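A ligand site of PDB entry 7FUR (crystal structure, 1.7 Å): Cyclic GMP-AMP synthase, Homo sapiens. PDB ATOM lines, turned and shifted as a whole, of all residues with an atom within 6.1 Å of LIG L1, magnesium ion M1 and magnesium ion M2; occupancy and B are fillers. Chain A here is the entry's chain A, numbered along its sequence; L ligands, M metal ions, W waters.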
ATOM      1  N   LEU A  49      -5.578 -35.277  -9.620  1.00  0.00           N
ATOM      2  CA  LEU A  49      -4.231 -34.759  -9.823  1.00  0.00           C
ATOM      3  C   LEU A  49      -4.000 -33.714  -8.746  1.00  0.00           C
ATOM      4  O   LEU A  49      -4.659 -32.664  -8.743  1.00  0.00           O
ATOM      5  CB  LEU A  49      -4.082 -34.172 -11.221  1.00  0.00           C
ATOM      6  CG  LEU A  49      -2.714 -34.256 -11.898  1.00  0.00           C
ATOM      7  CD1 LEU A  49      -2.807 -33.686 -13.305  1.00  0.00           C
ATOM      8  CD2 LEU A  49      -1.641 -33.531 -11.102  1.00  0.00           C
ATOM      9  N   THR A  51      -2.094 -30.748  -6.841  1.00  0.00           N
ATOM     10  CA  THR A  51      -1.310 -29.608  -7.318  1.00  0.00           C
ATOM     11  C   THR A  51      -1.210 -28.539  -6.222  1.00  0.00           C
ATOM     12  O   THR A  51      -1.813 -28.646  -5.147  1.00  0.00           O
ATOM     13  CB  THR A  51      -1.943 -29.002  -8.567  1.00  0.00           C
ATOM     14  OG1 THR A  51      -3.258 -28.545  -8.209  1.00  0.00           O
ATOM     15  CG2 THR A  51      -2.046 -30.015  -9.695  1.00  0.00           C
ATOM     16  N   GLY A  52      -0.477 -27.464  -6.534  1.00  0.00           N
ATOM     17  CA  GLY A  52      -0.436 -26.335  -5.624  1.00  0.00           C
ATOM     18  C   GLY A  52       0.501 -26.572  -4.461  1.00  0.00           C
ATOM     19  O   GLY A  52       1.188 -27.600  -4.362  1.00  0.00           O
ATOM     20  N   SER A  53       0.512 -25.598  -3.546  1.00  0.00           N
ATOM     21  CA  SER A  53       1.601 -25.466  -2.593  1.00  0.00           C
ATOM     22  C   SER A  53       1.644 -26.594  -1.554  1.00  0.00           C
ATOM     23  O   SER A  53       2.731 -26.935  -1.070  1.00  0.00           O
ATOM     24  CB  SER A  53       1.506 -24.120  -1.885  1.00  0.00           C
ATOM     25  OG  SER A  53       0.365 -24.059  -1.032  1.00  0.00           O
ATOM     26  N   TYR A  54       0.496 -27.148  -1.153  1.00  0.00           N
ATOM     27  CA  TYR A  54       0.558 -28.234  -0.179  1.00  0.00           C
ATOM     28  C   TYR A  54       1.348 -29.418  -0.731  1.00  0.00           C
ATOM     29  O   TYR A  54       2.201 -29.978  -0.032  1.00  0.00           O
ATOM     30  CB  TYR A  54      -0.844 -28.704   0.227  1.00  0.00           C
ATOM     31  CG  TYR A  54      -0.825 -29.888   1.193  1.00  0.00           C
ATOM     32  CD1 TYR A  54      -0.588 -29.702   2.548  1.00  0.00           C
ATOM     33  CD2 TYR A  54      -1.079 -31.189   0.752  1.00  0.00           C
ATOM     34  CE1 TYR A  54      -0.586 -30.777   3.423  1.00  0.00           C
ATOM     35  CE2 TYR A  54      -1.064 -32.261   1.621  1.00  0.00           C
ATOM     36  CZ  TYR A  54      -0.817 -32.055   2.957  1.00  0.00           C
ATOM     37  OH  TYR A  54      -0.839 -33.129   3.830  1.00  0.00           O
ATOM     38  N   LYS A  59       3.511 -24.848   1.111  1.00  0.00           N
ATOM     39  CA  LYS A  59       2.433 -24.227   1.886  1.00  0.00           C
ATOM     40  C   LYS A  59       2.981 -23.707   3.209  1.00  0.00           C
ATOM     41  O   LYS A  59       3.702 -24.416   3.917  1.00  0.00           O
ATOM     42  CB  LYS A  59       1.308 -25.242   2.158  1.00  0.00           C
ATOM     43  CG  LYS A  59       0.081 -24.647   2.894  1.00  0.00           C
ATOM     44  CD  LYS A  59      -0.831 -23.916   1.902  1.00  0.00           C
ATOM     45  CE  LYS A  59      -1.963 -23.167   2.621  1.00  0.00           C
ATOM     46  NZ  LYS A  59      -1.474 -22.096   3.578  1.00  0.00           N
ATOM     47  N   GLU A  65      -5.491 -24.751   2.874  1.00  0.00           N
ATOM     48  CA  GLU A  65      -5.877 -24.513   1.485  1.00  0.00           C
ATOM     49  C   GLU A  65      -5.238 -25.557   0.586  1.00  0.00           C
ATOM     50  O   GLU A  65      -4.008 -25.667   0.523  1.00  0.00           O
ATOM     51  CB  GLU A  65      -5.485 -23.104   1.019  1.00  0.00           C
ATOM     52  CG  GLU A  65      -6.341 -22.602  -0.150  1.00  0.00           C
ATOM     53  CD  GLU A  65      -5.723 -22.840  -1.533  1.00  0.00           C
ATOM     54  OE1 GLU A  65      -4.570 -23.310  -1.644  1.00  0.00           O
ATOM     55  OE2 GLU A  65      -6.416 -22.533  -2.534  1.00  0.00           O
ATOM     56  N   PHE A  66      -6.079 -26.294  -0.144  1.00  0.00           N
ATOM     57  CA  PHE A  66      -5.622 -27.388  -0.983  1.00  0.00           C
ATOM     58  C   PHE A  66      -6.101 -27.152  -2.408  1.00  0.00           C
ATOM     59  O   PHE A  66      -7.185 -26.608  -2.623  1.00  0.00           O
ATOM     60  CB  PHE A  66      -6.145 -28.736  -0.490  1.00  0.00           C
ATOM     61  CG  PHE A  66      -5.625 -29.141   0.855  1.00  0.00           C
ATOM     62  CD1 PHE A  66      -6.023 -28.476   2.021  1.00  0.00           C
ATOM     63  CD2 PHE A  66      -4.762 -30.218   0.972  1.00  0.00           C
ATOM     64  CE1 PHE A  66      -5.559 -28.878   3.269  1.00  0.00           C
ATOM     65  CE2 PHE A  66      -4.294 -30.629   2.223  1.00  0.00           C
ATOM     66  CZ  PHE A  66      -4.699 -29.960   3.373  1.00  0.00           C
ATOM     67  N   ASP A  67      -5.320 -27.627  -3.379  1.00  0.00           N
ATOM     68  CA  ASP A  67      -5.681 -27.450  -4.781  1.00  0.00           C
ATOM     69  C   ASP A  67      -5.617 -28.809  -5.458  1.00  0.00           C
ATOM     70  O   ASP A  67      -4.570 -29.474  -5.426  1.00  0.00           O
ATOM     71  CB  ASP A  67      -4.740 -26.460  -5.485  1.00  0.00           C
ATOM     72  CG  ASP A  67      -4.707 -25.129  -4.800  1.00  0.00           C
ATOM     73  OD1 ASP A  67      -5.656 -24.341  -4.978  1.00  0.00           O
ATOM     74  OD2 ASP A  67      -3.727 -24.880  -4.044  1.00  0.00           O
ATOM     75  N   VAL A  68      -6.723 -29.231  -6.051  1.00  0.00           N
ATOM     76  CA  VAL A  68      -6.714 -30.501  -6.768  1.00  0.00           C
ATOM     77  C   VAL A  68      -7.370 -30.287  -8.123  1.00  0.00           C
ATOM     78  O   VAL A  68      -8.300 -29.493  -8.270  1.00  0.00           O
ATOM     79  CB  VAL A  68      -7.413 -31.641  -5.987  1.00  0.00           C
ATOM     80  CG1 VAL A  68      -6.751 -31.902  -4.645  1.00  0.00           C
ATOM     81  CG2 VAL A  68      -8.850 -31.300  -5.767  1.00  0.00           C
ATOM     82  N   MET A  69      -6.863 -31.008  -9.112  1.00  0.00           N
ATOM     83  CA  MET A  69      -7.466 -31.042 -10.428  1.00  0.00           C
ATOM     84  C   MET A  69      -8.202 -32.350 -10.572  1.00  0.00           C
ATOM     85  O   MET A  69      -7.717 -33.397 -10.133  1.00  0.00           O
ATOM     86  CB  MET A  69      -6.426 -30.925 -11.539  1.00  0.00           C
ATOM     87  CG  MET A  69      -5.829 -29.531 -11.682  1.00  0.00           C
ATOM     88  SD  MET A  69      -4.551 -29.432 -12.952  1.00  0.00           S
ATOM     89  CE  MET A  69      -4.991 -30.835 -13.951  1.00  0.00           C
ATOM     90  N   TYR A  88      -5.176 -18.760 -23.956  1.00  0.00           N
ATOM     91  CA  TYR A  88      -6.570 -19.164 -24.031  1.00  0.00           C
ATOM     92  C   TYR A  88      -6.899 -19.768 -25.389  1.00  0.00           C
ATOM     93  O   TYR A  88      -6.421 -19.295 -26.431  1.00  0.00           O
ATOM     94  CB  TYR A  88      -7.495 -17.985 -23.775  1.00  0.00           C
ATOM     95  CG  TYR A  88      -7.318 -17.440 -22.386  1.00  0.00           C
ATOM     96  CD1 TYR A  88      -6.352 -16.485 -22.120  1.00  0.00           C
ATOM     97  CD2 TYR A  88      -8.098 -17.895 -21.344  1.00  0.00           C
ATOM     98  CE1 TYR A  88      -6.178 -15.985 -20.862  1.00  0.00           C
ATOM     99  CE2 TYR A  88      -7.943 -17.412 -20.082  1.00  0.00           C
ATOM    100  CZ  TYR A  88      -6.985 -16.437 -19.846  1.00  0.00           C
ATOM    101  OH  TYR A  88      -6.827 -15.956 -18.559  1.00  0.00           O
ATOM    102  N   LYS A 141     -15.815 -17.018  -5.177  1.00  0.00           N
ATOM    103  CA  LYS A 141     -15.177 -15.750  -4.873  1.00  0.00           C
ATOM    104  C   LYS A 141     -15.499 -14.745  -5.960  1.00  0.00           C
ATOM    105  O   LYS A 141     -16.583 -14.158  -5.977  1.00  0.00           O
ATOM    106  CB  LYS A 141     -13.668 -15.933  -4.737  1.00  0.00           C
ATOM    107  CG  LYS A 141     -13.274 -16.917  -3.673  1.00  0.00           C
ATOM    108  CD  LYS A 141     -11.774 -17.091  -3.634  1.00  0.00           C
ATOM    109  CE  LYS A 141     -11.369 -17.966  -2.454  1.00  0.00           C
ATOM    110  NZ  LYS A 141      -9.897 -18.183  -2.412  1.00  0.00           N
ATOM    111  N   SER A 145     -12.120 -17.650 -11.425  1.00  0.00           N
ATOM    112  CA  SER A 145     -11.348 -18.853 -11.144  1.00  0.00           C
ATOM    113  C   SER A 145     -11.895 -20.014 -11.971  1.00  0.00           C
ATOM    114  O   SER A 145     -13.097 -20.088 -12.219  1.00  0.00           O
ATOM    115  CB  SER A 145     -11.405 -19.230  -9.659  1.00  0.00           C
ATOM    116  OG  SER A 145     -10.628 -20.395  -9.404  1.00  0.00           O
ATOM    117  N   PRO A 146     -11.025 -20.923 -12.429  1.00  0.00           N
ATOM    118  CA  PRO A 146     -11.522 -22.157 -13.061  1.00  0.00           C
ATOM    119  C   PRO A 146     -12.012 -23.188 -12.062  1.00  0.00           C
ATOM    120  O   PRO A 146     -12.520 -24.234 -12.487  1.00  0.00           O
ATOM    121  CB  PRO A 146     -10.293 -22.668 -13.818  1.00  0.00           C
ATOM    122  CG  PRO A 146      -9.153 -22.234 -12.960  1.00  0.00           C
ATOM    123  CD  PRO A 146      -9.552 -20.917 -12.326  1.00  0.00           C
ATOM    124  N   ALA A 147     -11.900 -22.932 -10.757  1.00  0.00           N
ATOM    125  CA  ALA A 147     -12.193 -23.923  -9.730  1.00  0.00           C
ATOM    126  C   ALA A 147     -13.585 -23.789  -9.141  1.00  0.00           C
ATOM    127  O   ALA A 147     -14.185 -22.701  -9.124  1.00  0.00           O
ATOM    128  CB  ALA A 147     -11.183 -23.825  -8.586  1.00  0.00           C
ATOM    129  N   ASP A 159      -9.820 -25.982  -3.663  1.00  0.00           N
ATOM    130  CA  ASP A 159     -10.128 -25.630  -5.038  1.00  0.00           C
ATOM    131  C   ASP A 159     -10.150 -26.921  -5.848  1.00  0.00           C
ATOM    132  O   ASP A 159      -9.165 -27.652  -5.874  1.00  0.00           O
ATOM    133  CB  ASP A 159      -9.078 -24.679  -5.612  1.00  0.00           C
ATOM    134  CG  ASP A 159      -9.184 -23.285  -5.019  1.00  0.00           C
ATOM    135  OD1 ASP A 159     -10.324 -22.801  -4.813  1.00  0.00           O
ATOM    136  OD2 ASP A 159      -8.125 -22.679  -4.759  1.00  0.00           O
ATOM    137  N   ILE A 160     -11.299 -27.191  -6.473  1.00  0.00           N
ATOM    138  CA  ILE A 160     -11.478 -28.372  -7.311  1.00  0.00           C
ATOM    139  C   ILE A 160     -11.644 -27.880  -8.734  1.00  0.00           C
ATOM    140  O   ILE A 160     -12.622 -27.173  -9.053  1.00  0.00           O
ATOM    141  CB  ILE A 160     -12.670 -29.206  -6.860  1.00  0.00           C
ATOM    142  CG1 ILE A 160     -12.418 -29.713  -5.447  1.00  0.00           C
ATOM    143  CG2 ILE A 160     -12.900 -30.339  -7.833  1.00  0.00           C
ATOM    144  CD1 ILE A 160     -13.672 -29.877  -4.701  1.00  0.00           C
ATOM    145  N   THR A 161     -10.702 -28.223  -9.595  1.00  0.00           N
ATOM    146  CA  THR A 161     -10.637 -27.669 -10.930  1.00  0.00           C
ATOM    147  C   THR A 161     -10.778 -28.770 -11.975  1.00  0.00           C
ATOM    148  O   THR A 161      -9.929 -29.651 -12.061  1.00  0.00           O
ATOM    149  CB  THR A 161      -9.326 -26.927 -11.125  1.00  0.00           C
ATOM    150  OG1 THR A 161      -9.271 -25.890 -10.138  1.00  0.00           O
ATOM    151  CG2 THR A 161      -9.265 -26.340 -12.489  1.00  0.00           C
ATOM    152  N   VAL A 200      -7.967 -25.747 -18.431  1.00  0.00           N
ATOM    153  CA  VAL A 200      -8.920 -25.510 -17.335  1.00  0.00           C
ATOM    154  C   VAL A 200      -9.980 -24.511 -17.793  1.00  0.00           C
ATOM    155  O   VAL A 200      -9.702 -23.673 -18.660  1.00  0.00           O
ATOM    156  CB  VAL A 200      -8.235 -25.000 -16.064  1.00  0.00           C
ATOM    157  CG1 VAL A 200      -7.178 -26.008 -15.561  1.00  0.00           C
ATOM    158  CG2 VAL A 200      -7.644 -23.606 -16.301  1.00  0.00           C
ATOM    159  N   LYS A 202     -11.133 -21.551 -17.490  1.00  0.00           N
ATOM    160  CA  LYS A 202     -11.021 -20.130 -17.230  1.00  0.00           C
ATOM    161  C   LYS A 202     -11.148 -19.424 -18.560  1.00  0.00           C
ATOM    162  O   LYS A 202     -10.456 -19.792 -19.513  1.00  0.00           O
ATOM    163  CB  LYS A 202      -9.685 -19.811 -16.538  1.00  0.00           C
ATOM    164  CG  LYS A 202      -9.516 -18.320 -16.269  1.00  0.00           C
ATOM    165  CD  LYS A 202      -8.240 -18.014 -15.481  1.00  0.00           C
ATOM    166  CE  LYS A 202      -7.981 -16.505 -15.463  1.00  0.00           C
ATOM    167  NZ  LYS A 202      -9.075 -15.729 -14.808  1.00  0.00           N
ATOM    168  N   ARG A 216      -8.156 -22.373 -20.771  1.00  0.00           N
ATOM    169  CA  ARG A 216      -6.811 -21.862 -20.521  1.00  0.00           C
ATOM    170  C   ARG A 216      -5.808 -22.982 -20.257  1.00  0.00           C
ATOM    171  O   ARG A 216      -6.116 -23.958 -19.568  1.00  0.00           O
ATOM    172  CB  ARG A 216      -6.784 -20.906 -19.345  1.00  0.00           C
ATOM    173  CG  ARG A 216      -5.417 -20.345 -19.203  1.00  0.00           C
ATOM    174  CD  ARG A 216      -5.326 -19.331 -18.160  1.00  0.00           C
ATOM    175  NE  ARG A 216      -3.921 -19.050 -17.961  1.00  0.00           N
ATOM    176  CZ  ARG A 216      -3.458 -17.917 -17.457  1.00  0.00           C
ATOM    177  NH1 ARG A 216      -2.151 -17.749 -17.315  1.00  0.00           N
ATOM    178  NH2 ARG A 216      -4.310 -16.950 -17.111  1.00  0.00           N
ATOM    179  N   LEU A 217      -4.595 -22.821 -20.797  1.00  0.00           N
ATOM    180  CA  LEU A 217      -3.533 -23.785 -20.604  1.00  0.00           C
ATOM    181  C   LEU A 217      -3.046 -23.776 -19.163  1.00  0.00           C
ATOM    182  O   LEU A 217      -2.956 -22.719 -18.524  1.00  0.00           O
ATOM    183  CB  LEU A 217      -2.344 -23.484 -21.505  1.00  0.00           C
ATOM    184  CG  LEU A 217      -2.456 -23.519 -23.021  1.00  0.00           C
ATOM    185  CD1 LEU A 217      -1.084 -23.234 -23.575  1.00  0.00           C
ATOM    186  CD2 LEU A 217      -2.956 -24.865 -23.514  1.00  0.00           C
ATOM    187  N   SER A 218      -2.699 -24.957 -18.663  1.00  0.00           N
ATOM    188  CA  SER A 218      -2.178 -25.099 -17.308  1.00  0.00           C
ATOM    189  C   SER A 218      -1.060 -26.120 -17.282  1.00  0.00           C
ATOM    190  O   SER A 218      -1.217 -27.234 -17.812  1.00  0.00           O
ATOM    191  CB  SER A 218      -3.263 -25.494 -16.307  1.00  0.00           C
ATOM    192  OG  SER A 218      -2.672 -25.718 -15.041  1.00  0.00           O
ATOM    193  N   PHE A 219       0.028 -25.779 -16.608  1.00  0.00           N
ATOM    194  CA  PHE A 219       1.141 -26.701 -16.416  1.00  0.00           C
ATOM    195  C   PHE A 219       1.407 -26.953 -14.929  1.00  0.00           C
ATOM    196  O   PHE A 219       2.538 -27.217 -14.501  1.00  0.00           O
ATOM    197  CB  PHE A 219       2.370 -26.175 -17.158  1.00  0.00           C
ATOM    198  CG  PHE A 219       2.154 -26.040 -18.615  1.00  0.00           C
ATOM    199  CD1 PHE A 219       2.350 -27.114 -19.466  1.00  0.00           C
ATOM    200  CD2 PHE A 219       1.691 -24.838 -19.154  1.00  0.00           C
ATOM    201  CE1 PHE A 219       2.116 -26.992 -20.840  1.00  0.00           C
ATOM    202  CE2 PHE A 219       1.440 -24.703 -20.505  1.00  0.00           C
ATOM    203  CZ  PHE A 219       1.652 -25.783 -21.358  1.00  0.00           C
ATOM    204  N   SER A 220       0.335 -26.938 -14.124  1.00  0.00           N
ATOM    205  CA  SER A 220       0.480 -27.061 -12.683  1.00  0.00           C
ATOM    206  C   SER A 220       1.203 -28.351 -12.269  1.00  0.00           C
ATOM    207  O   SER A 220       1.954 -28.362 -11.290  1.00  0.00           O
ATOM    208  CB  SER A 220      -0.916 -26.964 -12.069  1.00  0.00           C
ATOM    209  OG  SER A 220      -0.852 -26.740 -10.671  1.00  0.00           O
ATOM    210  N   SER A 275       0.116 -15.471  -4.729  1.00  0.00           N
ATOM    211  CA  SER A 275       1.308 -16.280  -4.524  1.00  0.00           C
ATOM    212  C   SER A 275       1.888 -16.778  -5.834  1.00  0.00           C
ATOM    213  O   SER A 275       3.077 -17.067  -5.917  1.00  0.00           O
ATOM    214  CB  SER A 275       1.004 -17.457  -3.602  1.00  0.00           C
ATOM    215  OG  SER A 275       0.006 -18.273  -4.187  1.00  0.00           O
HETATM  216  C1  LIG L   1      -7.636 -19.396  -8.516  1.00  0.00           C
HETATM  217  C2  LIG L   1      -5.534 -24.056 -11.327  1.00  0.00           C
HETATM  218  C3  LIG L   1      -6.692 -24.359 -10.603  1.00  0.00           C
HETATM  219  C4  LIG L   1      -4.488 -24.972 -11.240  1.00  0.00           C
HETATM  220  O1  LIG L   1      -6.492 -20.443  -4.516  1.00  0.00           O
HETATM  221  C5  LIG L   1      -6.924 -19.873  -5.735  1.00  0.00           C
HETATM  222  C6  LIG L   1      -6.608 -20.889  -6.816  1.00  0.00           C
HETATM  223  O2  LIG L   1      -6.050 -21.927  -6.499  1.00  0.00           O
HETATM  224  N1  LIG L   1      -6.943 -20.615  -8.093  1.00  0.00           N
HETATM  225  C7  LIG L   1      -6.653 -21.602  -9.123  1.00  0.00           C
HETATM  226  C8  LIG L   1      -6.260 -20.957 -10.426  1.00  0.00           C
HETATM  227  C9  LIG L   1      -5.733 -21.521 -11.675  1.00  0.00           C
HETATM  228  C10 LIG L   1      -5.568 -20.418 -12.524  1.00  0.00           C
HETATM  229  N2  LIG L   1      -5.954 -19.266 -11.860  1.00  0.00           N
HETATM  230  C11 LIG L   1      -6.368 -19.608 -10.599  1.00  0.00           C
HETATM  231  C12 LIG L   1      -6.851 -18.641  -9.574  1.00  0.00           C
HETATM  232  C13 LIG L   1      -5.077 -20.576 -13.824  1.00  0.00           C
HETATM  233 CL1  LIG L   1      -4.883 -19.203 -14.842  1.00  0.00          CL
HETATM  234  C14 LIG L   1      -4.760 -21.849 -14.269  1.00  0.00           C
HETATM  235 CL2  LIG L   1      -4.122 -22.092 -15.856  1.00  0.00          CL
HETATM  236  C15 LIG L   1      -4.915 -22.948 -13.450  1.00  0.00           C
HETATM  237  C16 LIG L   1      -5.416 -22.816 -12.151  1.00  0.00           C
HETATM  238  N3  LIG L   1      -6.831 -25.446  -9.834  1.00  0.00           N
HETATM  239  C17 LIG L   1      -5.812 -26.329  -9.753  1.00  0.00           C
HETATM  240  N4  LIG L   1      -5.976 -27.422  -8.974  1.00  0.00           N
HETATM  241  C18 LIG L   1      -4.602 -26.113 -10.462  1.00  0.00           C
HETATM  242  P1  LG2 L   2      -0.854 -21.012  -1.864  1.00  0.00           P
HETATM  243  O1  LG2 L   2      -2.116 -21.837  -2.006  1.00  0.00           O
HETATM  244  O2  LG2 L   2      -1.095 -19.537  -1.941  1.00  0.00           O
HETATM  245  O3  LG2 L   2       0.098 -21.425  -0.771  1.00  0.00           O
HETATM  246  P2  LG2 L   2      -0.623 -22.146  -4.503  1.00  0.00           P
HETATM  247  O4  LG2 L   2       0.511 -22.287  -5.519  1.00  0.00           O
HETATM  248  O5  LG2 L   2      -1.343 -23.403  -4.114  1.00  0.00           O
HETATM  249  O6  LG2 L   2       0.020 -21.397  -3.207  1.00  0.00           O
HETATM  250  P3  LG2 L   2      -3.265 -21.230  -5.439  1.00  0.00           P
HETATM  251  O7  LG2 L   2      -3.777 -19.802  -5.616  1.00  0.00           O
HETATM  252  O8  LG2 L   2      -3.963 -22.219  -4.542  1.00  0.00           O
HETATM  253  O9  LG2 L   2      -1.698 -21.040  -5.029  1.00  0.00           O
HETATM  254  O10 LG2 L   2      -3.164 -21.886  -6.907  1.00  0.00           O
HETATM  255  C1  LG2 L   2      -3.142 -23.293  -7.077  1.00  0.00           C
HETATM  256  C2  LG2 L   2      -2.432 -23.536  -8.412  1.00  0.00           C
HETATM  257  O11 LG2 L   2      -3.174 -22.857  -9.421  1.00  0.00           O
HETATM  258  C3  LG2 L   2      -1.053 -22.908  -8.488  1.00  0.00           C
HETATM  259  O12 LG2 L   2      -0.029 -23.776  -7.999  1.00  0.00           O
HETATM  260  C4  LG2 L   2      -0.890 -22.682  -9.977  1.00  0.00           C
HETATM  261  O13 LG2 L   2      -0.357 -23.885 -10.557  1.00  0.00           O
HETATM  262  C5  LG2 L   2      -2.310 -22.454 -10.481  1.00  0.00           C
HETATM  263  N1  LG2 L   2      -2.503 -21.011 -10.710  1.00  0.00           N
HETATM  264  C6  LG2 L   2      -2.951 -20.103  -9.831  1.00  0.00           C
HETATM  265  N2  LG2 L   2      -2.989 -18.880 -10.392  1.00  0.00           N
HETATM  266  C7  LG2 L   2      -2.539 -19.009 -11.661  1.00  0.00           C
HETATM  267  C8  LG2 L   2      -2.318 -18.114 -12.826  1.00  0.00           C
HETATM  268  N3  LG2 L   2      -2.570 -16.794 -12.718  1.00  0.00           N
HETATM  269  N4  LG2 L   2      -1.842 -18.673 -13.966  1.00  0.00           N
HETATM  270  C9  LG2 L   2      -1.580 -19.981 -14.083  1.00  0.00           C
HETATM  271  N5  LG2 L   2      -1.770 -20.835 -13.066  1.00  0.00           N
HETATM  272  C10 LG2 L   2      -2.228 -20.421 -11.874  1.00  0.00           C
HETATM  273 MG    MG M   1      -3.065 -23.316  -2.918  1.00  0.00          MG
HETATM  274 MG    MG M   2      -6.042 -22.478  -4.537  1.00  0.00          MG
HETATM  275  O   HOH W   1      -6.033 -16.220 -12.160  1.00  0.00           O
HETATM  276  O   HOH W   2      -6.316 -18.490  -2.378  1.00  0.00           O
HETATM  277  O   HOH W   3      -2.183 -24.710  -1.693  1.00  0.00           O
HETATM  278  O   HOH W   4     -10.031 -20.614  -6.593  1.00  0.00           O
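Within 4 Å of magnesium ion M2: Glu 65, Asp 67 and Asp 159.
The nearest printed residue that does not touch magnesium ion M2 is Phe 66 (4.7 Å).
Water W3 bridges OG of Ser 53 (2.7 Å) and O of Glu 65 (3.0 Å).
Water W4 bridges the side-chain carboxylate of Asp 159 (2.8 Å) and the side-chain hydroxyl of Ser 145 (2.9 Å).
The side-chain carboxylate (OE1) of Glu 65 is bound to magnesium ion M1 (2.0 Å).
O1 of LG2 L2 binds magnesium ion M1 (2.0 Å).
OD2 of Asp 67 is bound to magnesium ion M1, 2.0 Å away.
Magnesium ion M1 is bound by water W3 (2.1 Å).
O5 of LG2 L2 binds magnesium ion M1 (2.1 Å).
An oxygen (O8) of LG2 L2 binds magnesium ion M1 (2.2 Å).
The guanidinium group of Arg 216 sits at hydrogen-bond distance from the side-chain hydroxyl of Tyr 88.
OG of Ser 145 sits at hydrogen-bond distance from N of Ala 147 (3.1 Å).
The backbone NH (N) of Val 200 sits at hydrogen-bond distance from the backbone carbonyl oxygen (O) of Arg 216 (2.8 Å).
O of Ser 53 sits at hydrogen-bond distance from N of Lys 59.
The backbone carbonyl oxygen of Asp 159 sits at hydrogen-bond distance from the backbone NH of Val 68 (2.9 Å).
The backbone carbonyl oxygen of Val 68 sits at hydrogen-bond distance from the backbone NH of Thr 161, 3.0 Å away.
N of Ser 220 is in hydrogen-bond range of OG of Ser 218.
N of Thr 51 lies within hydrogen-bond range of O of Asp 67.
OG of Ser 53 touches magnesium ion M1 (3.98 Å).
Three residues have an atom within 4 Å of magnesium ion M1: Ser 53, Glu 65 and Asp 67.
The nearest printed residue that does not touch magnesium ion M1 is Gly 52 (4.8 Å).
Met 69 touches LIG L1.
Ser 145 touches LIG L1.
Pro 146 touches LIG L1.
Val 200 touches LIG L1 (CG2 to CL2, 3.9 Å).
Lys 202 touches LIG L1.
Arg 216 touches LIG L1 (CZ to CL1, 3.2 Å).
Leu 217 touches LIG L1 (O to CL2, 3.0 Å).
Ser 218 touches LIG L1.
OG of Ser 220 touches C18 of LIG L1, at 3.8 Å.
Hydrophobic or aromatic side chains within 4 Å of LIG L1: Met 69, Pro 146 and Val 200.
Of the 27 residues printed, 15 come within 4 Å of LIG L1.
Magnesium ion M2 is bound by OD1 of Asp 67 (2.0 Å), O2 of LIG L1 (2.0 Å), OE2 of Glu 65 (2.0 Å), O1 of LIG L1 (2.1 Å), O8 of LG2 L2 (2.1 Å) and OD2 of Asp 159 (2.1 Å).
Magnesium ion M2 has six donor atoms within binding distance.
The side-chain hydroxyl of Thr 161 sits at hydrogen-bond distance from a nitrogen (N3) of LIG L1 (2.5 Å).
The side-chain hydroxyl (OG1) of Thr 51 sits at hydrogen-bond distance from a nitrogen (N4) of LIG L1, 3.0 Å away.
The backbone NH of Ser 53 sits close to an oxygen (O5) of LG2 L2.
N4 of LIG L1 sits at hydrogen-bond distance from O of Val 68, 3.2 Å away.
OG of Ser 220 lies within hydrogen-bond range of O13 of LG2 L2 (2.9 Å).
OG of Ser 53 lies within hydrogen-bond range of O3 of LG2 L2.
The guanidinium group (NH1) of Arg 216 is in hydrogen-bond range of a nitrogen (N4) of LG2 L2 (3.5 Å).
An oxygen (O2) of LG2 L2 lies within hydrogen-bond range of the side-chain hydroxyl of Ser 275, at 2.8 Å.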
